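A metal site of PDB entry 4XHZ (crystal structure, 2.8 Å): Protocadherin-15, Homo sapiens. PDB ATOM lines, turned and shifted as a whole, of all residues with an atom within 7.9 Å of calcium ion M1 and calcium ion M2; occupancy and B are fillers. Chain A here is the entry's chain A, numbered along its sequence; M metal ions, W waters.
The backbone NH of Asp 107 lies within hydrogen-bond range of the side-chain carboxylate of Asp 140 (2.9 Å). The backbone NH (N) of Tyr 68 sits close to the side-chain carboxylate (OE1) of Glu 16 (3.1 Å). The side-chain carboxylate of Glu 16 sits close to the side-chain amide nitrogen of Asn 17. The backbone carbonyl oxygen (O) of Lys 103 sits at hydrogen-bond distance from the backbone NH (N) of Glu 16, at 3.1 Å.
Calcium ion M1 is bound by the side-chain carboxylate of Asp 107 (2.3 Å), the side-chain carboxylate of Glu 69 (2.3 Å), the side-chain carboxylate of Asp 67 (2.4 Å), water W1 (2.4 Å) and the side-chain carboxylate of Glu 16 (2.8 Å).
The side-chain carboxylate (OD1) of Asp 104 binds calcium ion M2. OD1 of Asp 107 binds calcium ion M2, at 2.3 Å. O of Met 105 binds calcium ion M2. Calcium ion M2 is bound by OE2 of Glu 69, 2.5 Å away. Calcium ion M2 is bound by OE2 of Glu 16 (2.6 Å). Calcium ion M2 is bound by OE1 of Glu 69 (2.8 Å). Calcium ion M2 has six donor atoms within binding distance.
Of the 17 residues printed, 5 come within 4 Å of calcium ion M2.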
ATOM      1  N   GLU A  16      22.038   4.895   6.341  1.00  0.00           N
ATOM      2  CA  GLU A  16      23.093   5.230   5.386  1.00  0.00           C
ATOM      3  C   GLU A  16      23.311   4.064   4.441  1.00  0.00           C
ATOM      4  O   GLU A  16      23.034   2.922   4.778  1.00  0.00           O
ATOM      5  CB  GLU A  16      24.394   5.618   6.096  1.00  0.00           C
ATOM      6  CG  GLU A  16      25.123   4.501   6.835  1.00  0.00           C
ATOM      7  CD  GLU A  16      26.580   4.868   7.127  1.00  0.00           C
ATOM      8  OE1 GLU A  16      27.273   5.331   6.196  1.00  0.00           O
ATOM      9  OE2 GLU A  16      27.023   4.705   8.277  1.00  0.00           O
ATOM     10  N   ASN A  17      23.793   4.359   3.235  1.00  0.00           N
ATOM     11  CA  ASN A  17      24.126   3.303   2.274  1.00  0.00           C
ATOM     12  C   ASN A  17      22.925   2.597   1.668  1.00  0.00           C
ATOM     13  O   ASN A  17      23.067   1.483   1.192  1.00  0.00           O
ATOM     14  CB  ASN A  17      25.051   2.255   2.909  1.00  0.00           C
ATOM     15  CG  ASN A  17      26.369   2.844   3.392  1.00  0.00           C
ATOM     16  OD1 ASN A  17      26.921   3.770   2.780  1.00  0.00           O
ATOM     17  ND2 ASN A  17      26.883   2.312   4.500  1.00  0.00           N
ATOM     18  N   LEU A  66      23.238   7.946   1.229  1.00  0.00           N
ATOM     19  CA  LEU A  66      23.755   8.758   2.323  1.00  0.00           C
ATOM     20  C   LEU A  66      24.941   8.088   2.984  1.00  0.00           C
ATOM     21  O   LEU A  66      25.068   6.857   2.949  1.00  0.00           O
ATOM     22  CB  LEU A  66      22.659   9.028   3.338  1.00  0.00           C
ATOM     23  CG  LEU A  66      21.527   9.854   2.740  1.00  0.00           C
ATOM     24  CD1 LEU A  66      20.352   9.968   3.707  1.00  0.00           C
ATOM     25  CD2 LEU A  66      22.051  11.225   2.375  1.00  0.00           C
ATOM     26  N   ASP A  67      25.808   8.897   3.597  1.00  0.00           N
ATOM     27  CA  ASP A  67      26.962   8.385   4.357  1.00  0.00           C
ATOM     28  C   ASP A  67      27.059   9.039   5.753  1.00  0.00           C
ATOM     29  O   ASP A  67      27.469  10.206   5.888  1.00  0.00           O
ATOM     30  CB  ASP A  67      28.251   8.607   3.550  1.00  0.00           C
ATOM     31  CG  ASP A  67      29.510   8.312   4.351  1.00  0.00           C
ATOM     32  OD1 ASP A  67      29.423   7.760   5.473  1.00  0.00           O
ATOM     33  OD2 ASP A  67      30.600   8.628   3.837  1.00  0.00           O
ATOM     34  N   TYR A  68      26.708   8.282   6.780  1.00  0.00           N
ATOM     35  CA  TYR A  68      26.739   8.792   8.145  1.00  0.00           C
ATOM     36  C   TYR A  68      28.044   9.530   8.480  1.00  0.00           C
ATOM     37  O   TYR A  68      28.053  10.644   9.027  1.00  0.00           O
ATOM     38  CB  TYR A  68      26.519   7.655   9.148  1.00  0.00           C
ATOM     39  CG  TYR A  68      26.479   8.155  10.563  1.00  0.00           C
ATOM     40  CD1 TYR A  68      27.660   8.385  11.274  1.00  0.00           C
ATOM     41  CD2 TYR A  68      25.277   8.434  11.187  1.00  0.00           C
ATOM     42  CE1 TYR A  68      27.624   8.869  12.566  1.00  0.00           C
ATOM     43  CE2 TYR A  68      25.237   8.906  12.474  1.00  0.00           C
ATOM     44  CZ  TYR A  68      26.410   9.137  13.153  1.00  0.00           C
ATOM     45  OH  TYR A  68      26.378   9.619  14.432  1.00  0.00           O
ATOM     46  N   GLU A  69      29.158   8.882   8.174  1.00  0.00           N
ATOM     47  CA  GLU A  69      30.473   9.385   8.533  1.00  0.00           C
ATOM     48  C   GLU A  69      30.873  10.653   7.767  1.00  0.00           C
ATOM     49  O   GLU A  69      31.833  11.323   8.114  1.00  0.00           O
ATOM     50  CB  GLU A  69      31.540   8.285   8.349  1.00  0.00           C
ATOM     51  CG  GLU A  69      31.631   7.275   9.491  1.00  0.00           C
ATOM     52  CD  GLU A  69      30.539   6.216   9.447  1.00  0.00           C
ATOM     53  OE1 GLU A  69      30.096   5.863   8.334  1.00  0.00           O
ATOM     54  OE2 GLU A  69      30.131   5.734  10.534  1.00  0.00           O
ATOM     55  N   ALA A  70      30.134  10.989   6.724  1.00  0.00           N
ATOM     56  CA  ALA A  70      30.505  12.100   5.880  1.00  0.00           C
ATOM     57  C   ALA A  70      30.020  13.416   6.451  1.00  0.00           C
ATOM     58  O   ALA A  70      30.369  14.495   5.945  1.00  0.00           O
ATOM     59  CB  ALA A  70      29.978  11.900   4.471  1.00  0.00           C
ATOM     60  N   LYS A 103      20.860   7.313   9.854  1.00  0.00           N
ATOM     61  CA  LYS A 103      21.214   6.288  10.838  1.00  0.00           C
ATOM     62  C   LYS A 103      22.552   5.655  10.521  1.00  0.00           C
ATOM     63  O   LYS A 103      22.790   5.223   9.377  1.00  0.00           O
ATOM     64  CB  LYS A 103      20.148   5.210  10.918  1.00  0.00           C
ATOM     65  CG  LYS A 103      20.383   4.284  12.095  1.00  0.00           C
ATOM     66  CD  LYS A 103      19.378   3.154  12.106  1.00  0.00           C
ATOM     67  CE  LYS A 103      19.376   2.488  13.462  1.00  0.00           C
ATOM     68  NZ  LYS A 103      18.933   1.088  13.324  1.00  0.00           N
ATOM     69  N   ASP A 104      23.425   5.588  11.528  1.00  0.00           N
ATOM     70  CA  ASP A 104      24.722   4.946  11.359  1.00  0.00           C
ATOM     71  C   ASP A 104      24.590   3.428  11.106  1.00  0.00           C
ATOM     72  O   ASP A 104      23.744   2.749  11.706  1.00  0.00           O
ATOM     73  CB  ASP A 104      25.608   5.234  12.584  1.00  0.00           C
ATOM     74  CG  ASP A 104      27.047   4.784  12.383  1.00  0.00           C
ATOM     75  OD1 ASP A 104      27.424   4.340  11.271  1.00  0.00           O
ATOM     76  OD2 ASP A 104      27.824   4.884  13.342  1.00  0.00           O
ATOM     77  N   MET A 105      25.403   2.890  10.193  1.00  0.00           N
ATOM     78  CA  MET A 105      25.372   1.454   9.890  1.00  0.00           C
ATOM     79  C   MET A 105      26.781   0.903   9.799  1.00  0.00           C
ATOM     80  O   MET A 105      27.760   1.657   9.721  1.00  0.00           O
ATOM     81  CB  MET A 105      24.639   1.184   8.575  1.00  0.00           C
ATOM     82  CG  MET A 105      23.206   1.663   8.563  1.00  0.00           C
ATOM     83  SD  MET A 105      22.024   0.427   9.132  1.00  0.00           S
ATOM     84  CE  MET A 105      21.696   0.938  10.818  1.00  0.00           C
ATOM     85  N   ASN A 106      26.888  -0.412   9.814  1.00  0.00           N
ATOM     86  CA  ASN A 106      28.184  -1.045   9.696  1.00  0.00           C
ATOM     87  C   ASN A 106      28.709  -0.865   8.242  1.00  0.00           C
ATOM     88  O   ASN A 106      28.009  -1.213   7.290  1.00  0.00           O
ATOM     89  CB  ASN A 106      28.069  -2.514  10.148  1.00  0.00           C
ATOM     90  CG  ASN A 106      29.257  -3.360   9.762  1.00  0.00           C
ATOM     91  OD1 ASN A 106      30.406  -3.087  10.148  1.00  0.00           O
ATOM     92  ND2 ASN A 106      28.993  -4.437   9.018  1.00  0.00           N
ATOM     93  N   ASP A 107      29.910  -0.304   8.079  1.00  0.00           N
ATOM     94  CA  ASP A 107      30.442   0.001   6.735  1.00  0.00           C
ATOM     95  C   ASP A 107      31.364  -1.050   6.119  1.00  0.00           C
ATOM     96  O   ASP A 107      31.266  -1.359   4.925  1.00  0.00           O
ATOM     97  CB  ASP A 107      31.142   1.355   6.712  1.00  0.00           C
ATOM     98  CG  ASP A 107      30.180   2.495   6.744  1.00  0.00           C
ATOM     99  OD1 ASP A 107      29.453   2.620   7.748  1.00  0.00           O
ATOM    100  OD2 ASP A 107      30.124   3.267   5.768  1.00  0.00           O
ATOM    101  N   TYR A 108      32.275  -1.592   6.917  1.00  0.00           N
ATOM    102  CA  TYR A 108      33.313  -2.457   6.383  1.00  0.00           C
ATOM    103  C   TYR A 108      33.290  -3.867   6.922  1.00  0.00           C
ATOM    104  O   TYR A 108      32.925  -4.092   8.092  1.00  0.00           O
ATOM    105  CB  TYR A 108      34.679  -1.854   6.651  1.00  0.00           C
ATOM    106  CG  TYR A 108      34.763  -0.385   6.408  1.00  0.00           C
ATOM    107  CD1 TYR A 108      34.785   0.123   5.114  1.00  0.00           C
ATOM    108  CD2 TYR A 108      34.822   0.513   7.472  1.00  0.00           C
ATOM    109  CE1 TYR A 108      34.880   1.481   4.890  1.00  0.00           C
ATOM    110  CE2 TYR A 108      34.909   1.867   7.247  1.00  0.00           C
ATOM    111  CZ  TYR A 108      34.935   2.346   5.960  1.00  0.00           C
ATOM    112  OH  TYR A 108      35.023   3.694   5.744  1.00  0.00           O
ATOM    113  N   ASP A 140      35.674  -0.266  11.029  1.00  0.00           N
ATOM    114  CA  ASP A 140      34.613   0.497  11.707  1.00  0.00           C
ATOM    115  C   ASP A 140      35.057   1.004  13.094  1.00  0.00           C
ATOM    116  O   ASP A 140      35.979   0.455  13.695  1.00  0.00           O
ATOM    117  CB  ASP A 140      33.349  -0.338  11.838  1.00  0.00           C
ATOM    118  CG  ASP A 140      32.664  -0.585  10.494  1.00  0.00           C
ATOM    119  OD1 ASP A 140      31.934   0.312  10.027  1.00  0.00           O
ATOM    120  OD2 ASP A 140      32.863  -1.671   9.922  1.00  0.00           O
ATOM    121  N   PRO A 141      34.390   2.064  13.590  1.00  0.00           N
ATOM    122  CA  PRO A 141      34.631   2.618  14.927  1.00  0.00           C
ATOM    123  C   PRO A 141      34.976   1.536  15.951  1.00  0.00           C
ATOM    124  O   PRO A 141      34.182   0.615  16.167  1.00  0.00           O
ATOM    125  CB  PRO A 141      33.269   3.262  15.287  1.00  0.00           C
ATOM    126  CG  PRO A 141      32.358   3.031  14.095  1.00  0.00           C
ATOM    127  CD  PRO A 141      33.258   2.738  12.935  1.00  0.00           C
ATOM    128  N   ALA A 146      30.167  -3.498  15.703  1.00  0.00           N
ATOM    129  CA  ALA A 146      30.388  -3.481  14.263  1.00  0.00           C
ATOM    130  C   ALA A 146      31.882  -3.623  13.874  1.00  0.00           C
ATOM    131  O   ALA A 146      32.215  -3.844  12.703  1.00  0.00           O
ATOM    132  CB  ALA A 146      29.795  -2.224  13.635  1.00  0.00           C
ATOM    133  N   GLU A 199      25.110  -3.936  11.960  1.00  0.00           N
ATOM    134  CA  GLU A 199      23.880  -3.936  11.194  1.00  0.00           C
ATOM    135  C   GLU A 199      24.317  -3.525   9.793  1.00  0.00           C
ATOM    136  O   GLU A 199      24.779  -2.344   9.610  1.00  0.00           O
ATOM    137  CB  GLU A 199      22.897  -3.001  11.803  1.00  0.00           C
ATOM    138  CG  GLU A 199      21.571  -3.659  12.148  1.00  0.00           C
ATOM    139  CD  GLU A 199      20.628  -2.657  12.776  1.00  0.00           C
ATOM    140  OE1 GLU A 199      21.104  -1.842  13.603  1.00  0.00           O
ATOM    141  OE2 GLU A 199      19.434  -2.644  12.420  1.00  0.00           O
HETATM  142 CA    CA M   1      30.025   5.540   6.027  1.00  0.00          CA
HETATM  143 CA    CA M   2      28.936   3.671   9.707  1.00  0.00          CA
HETATM  144  O   HOH W   1      28.850   5.137   4.008  1.00  0.00           O
